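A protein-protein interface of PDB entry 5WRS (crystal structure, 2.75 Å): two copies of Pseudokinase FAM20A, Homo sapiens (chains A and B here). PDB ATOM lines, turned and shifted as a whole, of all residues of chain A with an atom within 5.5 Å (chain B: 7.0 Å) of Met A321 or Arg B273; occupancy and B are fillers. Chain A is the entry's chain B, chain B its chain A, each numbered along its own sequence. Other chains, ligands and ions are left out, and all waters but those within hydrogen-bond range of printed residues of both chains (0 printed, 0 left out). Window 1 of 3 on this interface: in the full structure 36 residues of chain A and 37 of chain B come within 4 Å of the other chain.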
ATOM      1  N   PHE A 166      13.127 -30.250  16.453  1.00  0.00           N
ATOM      2  CA  PHE A 166      12.062 -30.010  17.417  1.00  0.00           C
ATOM      3  C   PHE A 166      12.494 -30.290  18.849  1.00  0.00           C
ATOM      4  O   PHE A 166      11.697 -30.096  19.772  1.00  0.00           O
ATOM      5  CB  PHE A 166      10.829 -30.861  17.083  1.00  0.00           C
ATOM      6  CG  PHE A 166      10.128 -30.457  15.814  1.00  0.00           C
ATOM      7  CD1 PHE A 166      10.428 -29.261  15.183  1.00  0.00           C
ATOM      8  CD2 PHE A 166       9.164 -31.279  15.253  1.00  0.00           C
ATOM      9  CE1 PHE A 166       9.784 -28.894  14.016  1.00  0.00           C
ATOM     10  CE2 PHE A 166       8.515 -30.917  14.088  1.00  0.00           C
ATOM     11  CZ  PHE A 166       8.826 -29.723  13.468  1.00  0.00           C
ATOM     12  N   ILE A 272      -1.852 -18.696  16.747  1.00  0.00           N
ATOM     13  CA  ILE A 272      -0.901 -19.799  16.857  1.00  0.00           C
ATOM     14  C   ILE A 272      -0.480 -20.295  15.480  1.00  0.00           C
ATOM     15  O   ILE A 272       0.648 -20.775  15.301  1.00  0.00           O
ATOM     16  CB  ILE A 272      -1.502 -20.934  17.714  1.00  0.00           C
ATOM     17  CG1 ILE A 272      -0.491 -22.068  17.908  1.00  0.00           C
ATOM     18  CG2 ILE A 272      -2.788 -21.457  17.091  1.00  0.00           C
ATOM     19  CD1 ILE A 272       0.845 -21.615  18.457  1.00  0.00           C
ATOM     20  N   ARG A 273      -1.355 -20.176  14.487  1.00  0.00           N
ATOM     21  CA  ARG A 273      -1.081 -20.639  13.135  1.00  0.00           C
ATOM     22  C   ARG A 273      -1.170 -19.480  12.156  1.00  0.00           C
ATOM     23  O   ARG A 273      -1.938 -18.534  12.354  1.00  0.00           O
ATOM     24  CB  ARG A 273      -2.061 -21.746  12.709  1.00  0.00           C
ATOM     25  CG  ARG A 273      -2.259 -22.830  13.747  1.00  0.00           C
ATOM     26  CD  ARG A 273      -0.974 -23.600  13.996  1.00  0.00           C
ATOM     27  NE  ARG A 273      -0.835 -24.724  13.073  1.00  0.00           N
ATOM     28  CZ  ARG A 273      -0.155 -24.679  11.934  1.00  0.00           C
ATOM     29  NH1 ARG A 273       0.462 -23.563  11.565  1.00  0.00           N
ATOM     30  NH2 ARG A 273      -0.090 -25.755  11.162  1.00  0.00           N
ATOM     31  N   SER A 274      -0.367 -19.558  11.103  1.00  0.00           N
ATOM     32  CA  SER A 274      -0.466 -18.641   9.978  1.00  0.00           C
ATOM     33  C   SER A 274      -1.158 -19.345   8.816  1.00  0.00           C
ATOM     34  O   SER A 274      -1.237 -20.575   8.761  1.00  0.00           O
ATOM     35  CB  SER A 274       0.917 -18.137   9.557  1.00  0.00           C
ATOM     36  OG  SER A 274       1.806 -19.215   9.329  1.00  0.00           O
ATOM     37  N   GLY A 319      11.569 -16.095  20.194  1.00  0.00           N
ATOM     38  CA  GLY A 319      11.369 -17.048  19.119  1.00  0.00           C
ATOM     39  C   GLY A 319      10.569 -18.273  19.512  1.00  0.00           C
ATOM     40  O   GLY A 319      10.947 -19.403  19.186  1.00  0.00           O
ATOM     41  N   ASN A 320       9.453 -18.061  20.204  1.00  0.00           N
ATOM     42  CA  ASN A 320       8.606 -19.143  20.695  1.00  0.00           C
ATOM     43  C   ASN A 320       7.409 -19.293  19.762  1.00  0.00           C
ATOM     44  O   ASN A 320       6.495 -18.462  19.776  1.00  0.00           O
ATOM     45  CB  ASN A 320       8.156 -18.864  22.127  1.00  0.00           C
ATOM     46  CG  ASN A 320       7.192 -19.909  22.648  1.00  0.00           C
ATOM     47  OD1 ASN A 320       7.259 -21.075  22.265  1.00  0.00           O
ATOM     48  ND2 ASN A 320       6.285 -19.493  23.524  1.00  0.00           N
ATOM     49  N   MET A 321       7.421 -20.347  18.946  1.00  0.00           N
ATOM     50  CA  MET A 321       6.326 -20.647  18.033  1.00  0.00           C
ATOM     51  C   MET A 321       5.285 -21.578  18.640  1.00  0.00           C
ATOM     52  O   MET A 321       4.371 -22.008  17.931  1.00  0.00           O
ATOM     53  CB  MET A 321       6.860 -21.265  16.741  1.00  0.00           C
ATOM     54  CG  MET A 321       7.673 -20.324  15.874  1.00  0.00           C
ATOM     55  SD  MET A 321       8.359 -21.168  14.436  1.00  0.00           S
ATOM     56  CE  MET A 321       6.858 -21.577  13.543  1.00  0.00           C
ATOM     57  N   ASP A 322       5.397 -21.901  19.929  1.00  0.00           N
ATOM     58  CA  ASP A 322       4.585 -22.941  20.548  1.00  0.00           C
ATOM     59  C   ASP A 322       3.684 -22.401  21.654  1.00  0.00           C
ATOM     60  O   ASP A 322       3.391 -23.109  22.619  1.00  0.00           O
ATOM     61  CB  ASP A 322       5.471 -24.064  21.085  1.00  0.00           C
ATOM     62  CG  ASP A 322       6.096 -24.888  19.981  1.00  0.00           C
ATOM     63  OD1 ASP A 322       5.380 -25.728  19.396  1.00  0.00           O
ATOM     64  OD2 ASP A 322       7.298 -24.701  19.696  1.00  0.00           O
ATOM     65  N   ARG A 323       3.240 -21.150  21.537  1.00  0.00           N
ATOM     66  CA  ARG A 323       2.278 -20.597  22.491  1.00  0.00           C
ATOM     67  C   ARG A 323       0.860 -20.885  21.997  1.00  0.00           C
ATOM     68  O   ARG A 323       0.130 -20.014  21.517  1.00  0.00           O
ATOM     69  CB  ARG A 323       2.519 -19.108  22.701  1.00  0.00           C
ATOM     70  CG  ARG A 323       1.675 -18.502  23.814  1.00  0.00           C
ATOM     71  CD  ARG A 323       2.524 -17.657  24.735  1.00  0.00           C
ATOM     72  NE  ARG A 323       3.108 -18.439  25.818  1.00  0.00           N
ATOM     73  CZ  ARG A 323       4.257 -18.142  26.412  1.00  0.00           C
ATOM     74  NH1 ARG A 323       4.958 -17.089  26.012  1.00  0.00           N
ATOM     75  NH2 ARG A 323       4.716 -18.905  27.394  1.00  0.00           N
ATOM     76  N   HIS A 324       0.481 -22.158  22.122  1.00  0.00           N
ATOM     77  CA  HIS A 324      -0.844 -22.586  21.687  1.00  0.00           C
ATOM     78  C   HIS A 324      -1.941 -21.982  22.551  1.00  0.00           C
ATOM     79  O   HIS A 324      -3.028 -21.673  22.046  1.00  0.00           O
ATOM     80  CB  HIS A 324      -0.935 -24.113  21.712  1.00  0.00           C
ATOM     81  CG  HIS A 324       0.124 -24.793  20.903  1.00  0.00           C
ATOM     82  ND1 HIS A 324       1.343 -25.159  21.432  1.00  0.00           N
ATOM     83  CD2 HIS A 324       0.150 -25.169  19.603  1.00  0.00           C
ATOM     84  CE1 HIS A 324       2.073 -25.735  20.493  1.00  0.00           C
ATOM     85  NE2 HIS A 324       1.372 -25.754  19.373  1.00  0.00           N
ATOM     86  N   ARG A 345      10.152 -23.646  25.010  1.00  0.00           N
ATOM     87  CA  ARG A 345      10.351 -23.716  23.568  1.00  0.00           C
ATOM     88  C   ARG A 345      10.993 -22.456  22.999  1.00  0.00           C
ATOM     89  O   ARG A 345      11.124 -22.339  21.776  1.00  0.00           O
ATOM     90  CB  ARG A 345       9.017 -23.990  22.869  1.00  0.00           C
ATOM     91  CG  ARG A 345       8.194 -25.092  23.520  1.00  0.00           C
ATOM     92  CD  ARG A 345       8.656 -26.470  23.079  1.00  0.00           C
ATOM     93  NE  ARG A 345       8.744 -26.571  21.626  1.00  0.00           N
ATOM     94  CZ  ARG A 345       9.258 -27.610  20.976  1.00  0.00           C
ATOM     95  NH1 ARG A 345       9.733 -28.649  21.650  1.00  0.00           N
ATOM     96  NH2 ARG A 345       9.299 -27.609  19.651  1.00  0.00           N
ATOM     97  N   ARG A 349      16.569 -21.031  18.328  1.00  0.00           N
ATOM     98  CA  ARG A 349      17.217 -20.670  17.072  1.00  0.00           C
ATOM     99  C   ARG A 349      17.643 -19.213  17.164  1.00  0.00           C
ATOM    100  O   ARG A 349      16.799 -18.315  17.104  1.00  0.00           O
ATOM    101  CB  ARG A 349      16.297 -20.886  15.868  1.00  0.00           C
ATOM    102  CG  ARG A 349      15.965 -22.334  15.559  1.00  0.00           C
ATOM    103  CD  ARG A 349      15.202 -22.429  14.245  1.00  0.00           C
ATOM    104  NE  ARG A 349      14.541 -23.717  14.067  1.00  0.00           N
ATOM    105  CZ  ARG A 349      13.294 -23.973  14.445  1.00  0.00           C
ATOM    106  NH1 ARG A 349      12.568 -23.026  15.028  1.00  0.00           N
ATOM    107  NH2 ARG A 349      12.768 -25.174  14.240  1.00  0.00           N
ATOM    108  N   GLU A 354      11.205 -15.515  13.367  1.00  0.00           N
ATOM    109  CA  GLU A 354       9.908 -15.920  12.825  1.00  0.00           C
ATOM    110  C   GLU A 354       8.923 -14.773  13.010  1.00  0.00           C
ATOM    111  O   GLU A 354       8.233 -14.674  14.027  1.00  0.00           O
ATOM    112  CB  GLU A 354       9.422 -17.197  13.498  1.00  0.00           C
ATOM    113  CG  GLU A 354       8.250 -17.851  12.791  1.00  0.00           C
ATOM    114  CD  GLU A 354       8.358 -17.743  11.284  1.00  0.00           C
ATOM    115  OE1 GLU A 354       7.569 -16.983  10.683  1.00  0.00           O
ATOM    116  OE2 GLU A 354       9.248 -18.400  10.703  1.00  0.00           O
ATOM    117  N   SER A 356       6.135 -14.265  11.805  1.00  0.00           N
ATOM    118  CA  SER A 356       4.733 -14.656  11.919  1.00  0.00           C
ATOM    119  C   SER A 356       4.245 -14.629  13.361  1.00  0.00           C
ATOM    120  O   SER A 356       3.034 -14.541  13.592  1.00  0.00           O
ATOM    121  CB  SER A 356       4.529 -16.047  11.325  1.00  0.00           C
ATOM    122  OG  SER A 356       5.195 -17.028  12.099  1.00  0.00           O
ATOM    123  N   ILE A 357       5.155 -14.720  14.334  1.00  0.00           N
ATOM    124  CA  ILE A 357       4.760 -14.581  15.732  1.00  0.00           C
ATOM    125  C   ILE A 357       4.247 -13.172  16.000  1.00  0.00           C
ATOM    126  O   ILE A 357       3.310 -12.973  16.782  1.00  0.00           O
ATOM    127  CB  ILE A 357       5.933 -14.948  16.660  1.00  0.00           C
ATOM    128  CG1 ILE A 357       6.434 -16.358  16.348  1.00  0.00           C
ATOM    129  CG2 ILE A 357       5.506 -14.862  18.108  1.00  0.00           C
ATOM    130  CD1 ILE A 357       7.690 -16.742  17.094  1.00  0.00           C
ATOM    131  N   ASN B 269       5.491 -34.892  12.798  1.00  0.00           N
ATOM    132  CA  ASN B 269       5.453 -34.475  11.402  1.00  0.00           C
ATOM    133  C   ASN B 269       6.427 -33.321  11.197  1.00  0.00           C
ATOM    134  O   ASN B 269       6.196 -32.217  11.706  1.00  0.00           O
ATOM    135  CB  ASN B 269       4.026 -34.069  11.019  1.00  0.00           C
ATOM    136  CG  ASN B 269       3.919 -33.514   9.611  1.00  0.00           C
ATOM    137  OD1 ASN B 269       4.829 -33.659   8.794  1.00  0.00           O
ATOM    138  ND2 ASN B 269       2.796 -32.865   9.321  1.00  0.00           N
ATOM    139  N   PRO B 270       7.527 -33.533  10.466  1.00  0.00           N
ATOM    140  CA  PRO B 270       8.519 -32.457  10.294  1.00  0.00           C
ATOM    141  C   PRO B 270       7.999 -31.239   9.543  1.00  0.00           C
ATOM    142  O   PRO B 270       8.670 -30.199   9.556  1.00  0.00           O
ATOM    143  CB  PRO B 270       9.653 -33.143   9.516  1.00  0.00           C
ATOM    144  CG  PRO B 270       9.463 -34.606   9.772  1.00  0.00           C
ATOM    145  CD  PRO B 270       7.981 -34.801   9.873  1.00  0.00           C
ATOM    146  N   TRP B 271       6.839 -31.328   8.891  1.00  0.00           N
ATOM    147  CA  TRP B 271       6.269 -30.211   8.150  1.00  0.00           C
ATOM    148  C   TRP B 271       5.009 -29.663   8.811  1.00  0.00           C
ATOM    149  O   TRP B 271       4.207 -28.995   8.149  1.00  0.00           O
ATOM    150  CB  TRP B 271       5.966 -30.627   6.710  1.00  0.00           C
ATOM    151  CG  TRP B 271       7.176 -30.769   5.849  1.00  0.00           C
ATOM    152  CD1 TRP B 271       7.760 -29.799   5.089  1.00  0.00           C
ATOM    153  CD2 TRP B 271       7.957 -31.954   5.657  1.00  0.00           C
ATOM    154  NE1 TRP B 271       8.856 -30.306   4.433  1.00  0.00           N
ATOM    155  CE2 TRP B 271       8.998 -31.628   4.765  1.00  0.00           C
ATOM    156  CE3 TRP B 271       7.876 -33.261   6.150  1.00  0.00           C
ATOM    157  CZ2 TRP B 271       9.952 -32.559   4.356  1.00  0.00           C
ATOM    158  CZ3 TRP B 271       8.824 -34.183   5.745  1.00  0.00           C
ATOM    159  CH2 TRP B 271       9.847 -33.829   4.856  1.00  0.00           C
ATOM    160  N   ILE B 272       4.818 -29.933  10.106  1.00  0.00           N
ATOM    161  CA  ILE B 272       3.642 -29.427  10.809  1.00  0.00           C
ATOM    162  C   ILE B 272       3.638 -27.904  10.840  1.00  0.00           C
ATOM    163  O   ILE B 272       2.571 -27.277  10.857  1.00  0.00           O
ATOM    164  CB  ILE B 272       3.568 -30.027  12.229  1.00  0.00           C
ATOM    165  CG1 ILE B 272       2.286 -29.584  12.938  1.00  0.00           C
ATOM    166  CG2 ILE B 272       4.785 -29.631  13.052  1.00  0.00           C
ATOM    167  CD1 ILE B 272       1.024 -29.870  12.154  1.00  0.00           C
ATOM    168  N   ARG B 273       4.814 -27.281  10.828  1.00  0.00           N
ATOM    169  CA  ARG B 273       4.920 -25.832  10.876  1.00  0.00           C
ATOM    170  C   ARG B 273       5.649 -25.327   9.639  1.00  0.00           C
ATOM    171  O   ARG B 273       6.549 -25.988   9.114  1.00  0.00           O
ATOM    172  CB  ARG B 273       5.664 -25.364  12.136  1.00  0.00           C
ATOM    173  CG  ARG B 273       5.220 -26.058  13.413  1.00  0.00           C
ATOM    174  CD  ARG B 273       3.763 -25.776  13.740  1.00  0.00           C
ATOM    175  NE  ARG B 273       3.599 -24.556  14.524  1.00  0.00           N
ATOM    176  CZ  ARG B 273       3.316 -23.367  14.004  1.00  0.00           C
ATOM    177  NH1 ARG B 273       3.159 -23.233  12.691  1.00  0.00           N
ATOM    178  NH2 ARG B 273       3.184 -22.314  14.800  1.00  0.00           N
ATOM    179  N   SER B 274       5.251 -24.144   9.184  1.00  0.00           N
ATOM    180  CA  SER B 274       5.949 -23.429   8.128  1.00  0.00           C
ATOM    181  C   SER B 274       6.759 -22.283   8.726  1.00  0.00           C
ATOM    182  O   SER B 274       6.520 -21.843   9.854  1.00  0.00           O
ATOM    183  CB  SER B 274       4.964 -22.901   7.080  1.00  0.00           C
ATOM    184  OG  SER B 274       3.926 -22.148   7.680  1.00  0.00           O
ATOM    185  N   TYR B 275       7.728 -21.803   7.952  1.00  0.00           N
ATOM    186  CA  TYR B 275       8.648 -20.773   8.408  1.00  0.00           C
ATOM    187  C   TYR B 275       8.756 -19.683   7.353  1.00  0.00           C
ATOM    188  O   TYR B 275       8.679 -19.948   6.150  1.00  0.00           O
ATOM    189  CB  TYR B 275      10.037 -21.355   8.714  1.00  0.00           C
ATOM    190  CG  TYR B 275      10.008 -22.493   9.710  1.00  0.00           C
ATOM    191  CD1 TYR B 275      10.068 -22.250  11.075  1.00  0.00           C
ATOM    192  CD2 TYR B 275       9.912 -23.812   9.285  1.00  0.00           C
ATOM    193  CE1 TYR B 275      10.037 -23.289  11.990  1.00  0.00           C
ATOM    194  CE2 TYR B 275       9.880 -24.856  10.192  1.00  0.00           C
ATOM    195  CZ  TYR B 275       9.943 -24.588  11.543  1.00  0.00           C
ATOM    196  OH  TYR B 275       9.912 -25.622  12.451  1.00  0.00           O
ATOM    197  N   THR B 276       8.918 -18.445   7.817  1.00  0.00           N
ATOM    198  CA  THR B 276       9.087 -17.297   6.928  1.00  0.00           C
ATOM    199  C   THR B 276      10.562 -17.183   6.569  1.00  0.00           C
ATOM    200  O   THR B 276      11.375 -16.707   7.365  1.00  0.00           O
ATOM    201  CB  THR B 276       8.579 -16.016   7.578  1.00  0.00           C
ATOM    202  OG1 THR B 276       7.205 -16.177   7.952  1.00  0.00           O
ATOM    203  CG2 THR B 276       8.699 -14.849   6.609  1.00  0.00           C
ATOM    204  N   TRP B 283       8.375 -20.604   1.289  1.00  0.00           N
ATOM    205  CA  TRP B 283       8.708 -21.769   2.104  1.00  0.00           C
ATOM    206  C   TRP B 283       8.370 -23.075   1.393  1.00  0.00           C
ATOM    207  O   TRP B 283       9.187 -24.003   1.358  1.00  0.00           O
ATOM    208  CB  TRP B 283       7.974 -21.681   3.441  1.00  0.00           C
ATOM    209  CG  TRP B 283       7.826 -22.991   4.150  1.00  0.00           C
ATOM    210  CD1 TRP B 283       6.690 -23.743   4.252  1.00  0.00           C
ATOM    211  CD2 TRP B 283       8.841 -23.700   4.870  1.00  0.00           C
ATOM    212  NE1 TRP B 283       6.937 -24.877   4.986  1.00  0.00           N
ATOM    213  CE2 TRP B 283       8.250 -24.875   5.377  1.00  0.00           C
ATOM    214  CE3 TRP B 283      10.194 -23.458   5.131  1.00  0.00           C
ATOM    215  CZ2 TRP B 283       8.964 -25.804   6.131  1.00  0.00           C
ATOM    216  CZ3 TRP B 283      10.900 -24.382   5.879  1.00  0.00           C
ATOM    217  CH2 TRP B 283      10.284 -25.539   6.370  1.00  0.00           C
ATOM    218  N   TYR B 289      15.018 -27.114   3.021  1.00  0.00           N
ATOM    219  CA  TYR B 289      14.550 -27.826   4.208  1.00  0.00           C
ATOM    220  C   TYR B 289      14.468 -29.328   3.961  1.00  0.00           C
ATOM    221  O   TYR B 289      14.983 -30.126   4.754  1.00  0.00           O
ATOM    222  CB  TYR B 289      13.196 -27.277   4.650  1.00  0.00           C
ATOM    223  CG  TYR B 289      12.687 -27.873   5.944  1.00  0.00           C
ATOM    224  CD1 TYR B 289      13.378 -27.689   7.134  1.00  0.00           C
ATOM    225  CD2 TYR B 289      11.514 -28.615   5.977  1.00  0.00           C
ATOM    226  CE1 TYR B 289      12.914 -28.230   8.321  1.00  0.00           C
ATOM    227  CE2 TYR B 289      11.041 -29.154   7.160  1.00  0.00           C
ATOM    228  CZ  TYR B 289      11.745 -28.960   8.327  1.00  0.00           C
ATOM    229  OH  TYR B 289      11.275 -29.501   9.503  1.00  0.00           O
ATOM    230  N   MET B 321      -4.796 -29.070   9.007  1.00  0.00           N
ATOM    231  CA  MET B 321      -3.582 -28.412   9.463  1.00  0.00           C
ATOM    232  C   MET B 321      -3.087 -28.953  10.796  1.00  0.00           C
ATOM    233  O   MET B 321      -2.120 -28.417  11.348  1.00  0.00           O
ATOM    234  CB  MET B 321      -3.818 -26.907   9.586  1.00  0.00           C
ATOM    235  CG  MET B 321      -4.061 -26.196   8.270  1.00  0.00           C
ATOM    236  SD  MET B 321      -4.456 -24.458   8.533  1.00  0.00           S
ATOM    237  CE  MET B 321      -2.900 -23.857   9.200  1.00  0.00           C
ATOM    238  N   HIS B 324      -0.106 -33.162  13.724  1.00  0.00           N
ATOM    239  CA  HIS B 324       1.129 -32.973  14.474  1.00  0.00           C
ATOM    240  C   HIS B 324       1.958 -34.248  14.509  1.00  0.00           C
ATOM    241  O   HIS B 324       3.192 -34.182  14.542  1.00  0.00           O
ATOM    242  CB  HIS B 324       0.808 -32.496  15.892  1.00  0.00           C
ATOM    243  CG  HIS B 324      -0.019 -31.249  15.936  1.00  0.00           C
ATOM    244  ND1 HIS B 324       0.535 -29.986  15.951  1.00  0.00           N
ATOM    245  CD2 HIS B 324      -1.362 -31.070  15.961  1.00  0.00           C
ATOM    246  CE1 HIS B 324      -0.430 -29.084  15.986  1.00  0.00           C
ATOM    247  NE2 HIS B 324      -1.591 -29.715  15.993  1.00  0.00           N
ATOM    248  N   SER B 356       0.506 -24.779   2.443  1.00  0.00           N
ATOM    249  CA  SER B 356       1.615 -25.159   3.310  1.00  0.00           C
ATOM    250  C   SER B 356       1.511 -26.608   3.767  1.00  0.00           C
ATOM    251  O   SER B 356       2.524 -27.198   4.158  1.00  0.00           O
ATOM    252  CB  SER B 356       1.681 -24.234   4.525  1.00  0.00           C
ATOM    253  OG  SER B 356       0.559 -24.421   5.366  1.00  0.00           O
ATOM    254  N   SER B 359       3.600 -28.859   1.628  1.00  0.00           N
ATOM    255  CA  SER B 359       5.033 -28.580   1.618  1.00  0.00           C
ATOM    256  C   SER B 359       5.917 -29.797   1.360  1.00  0.00           C
ATOM    257  O   SER B 359       6.889 -29.656   0.598  1.00  0.00           O
ATOM    258  CB  SER B 359       5.432 -27.901   2.937  1.00  0.00           C
ATOM    259  OG  SER B 359       4.930 -26.577   2.992  1.00  0.00           O
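O of Ile B272 sits at hydrogen-bond distance from NH2 of Arg A273 (3.1 Å).
NH2 of Arg B273 lies within hydrogen-bond range of O of Ile A272, at 3.0 Å.
The guanidinium group of Arg B273 is in hydrogen-bond range of the backbone carbonyl oxygen of Met A321 (3.4 Å).
NH2 of Arg A349 lies within hydrogen-bond range of OH of Tyr B275.
OE1 of Glu A354 lies within hydrogen-bond range of OG1 of Thr B276 (2.9 Å).
The guanidinium group (NH2) of Arg A273 is in hydrogen-bond range of the backbone carbonyl oxygen (O) of Met B321, 3.4 Å away.
The guanidinium group (NH1) of Arg A273 sits close to the guanidinium group (NH1) of Arg B273, 2.9 Å away.
N of Trp B271 lies close to OD1 of Asn B269, at 3.1 Å.
The backbone NH (N) of Asn B269 sits at hydrogen-bond distance from the backbone carbonyl oxygen (O) of His B324 (3.0 Å).
The side-chain hydroxyl (OH) of Tyr B289 is in hydrogen-bond range of the backbone carbonyl oxygen (O) of Pro B270, 2.7 Å away.
NH1 of Arg A345 sits at hydrogen-bond distance from O of Phe A166 (3.1 Å).
The side-chain carboxylate of Glu A354 lies within hydrogen-bond range of the side-chain hydroxyl of Ser A356 (2.8 Å).
Among the printed residues, pairs that only touch across the chains: Phe A166 with Asn B269, Phe A166 with Pro B270, Phe A166 with Tyr B275, Ser A274 with Ser B274, Ser A274 with Met B321, Met A321 with Ser B274, Met A321 with Tyr B275 and Glu A354 with Tyr B275.
Of chain B, only Arg B273 (3.4 Å), Ser B274 (3.7 Å) and Tyr B275 (3.6 Å) come within 4 Å of Met A321.
Arg B273 touches just these residues of chain A: Ile A272, Arg A273 and Met A321.
Printed residues of chain A within 4 Å of Thr B276: Glu A354.
Of the printed residues of chain A, Tyr B275 touches Phe A166, Met A321, Arg A349 and Glu A354.
Of the printed residues of chain B, Arg A273 touches Ile B272, Arg B273 and Met B321.
Of the printed residues of chain A, Ser B274 touches Ser A274 and Met A321.
Of the printed residues of chain A, Asn B269 touches Phe A166 (3.6 Å).
Of the 15 printed residues of chain A, 7 touch a printed residue of chain B.
Hydrophobic or aromatic side chains of chain B that line the printed part of chain A: Tyr B275 and Met B321.
Along chain B the printed residues that touch a printed residue of chain A span positions 269 to 321.
Among the printed residues, no Asp or Glu carboxylate lies within 4 Å of a Lys or Arg side-chain nitrogen of the other chain.
Ile A272 touches Arg B273, and with the chains exchanged Arg A273 touches Ile B272.
Arg A273 touches its own counterpart, Arg B273.
Ser B274 touches its own counterpart, Ser A274.
Ser A274 touches Met B321, and with the chains exchanged Met A321 touches Ser B274.
6 positions are printed for both chains.
Of the 15 pairs that touch across the chains among the printed residues, 8 have their exchanged pair printed and touching as well.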
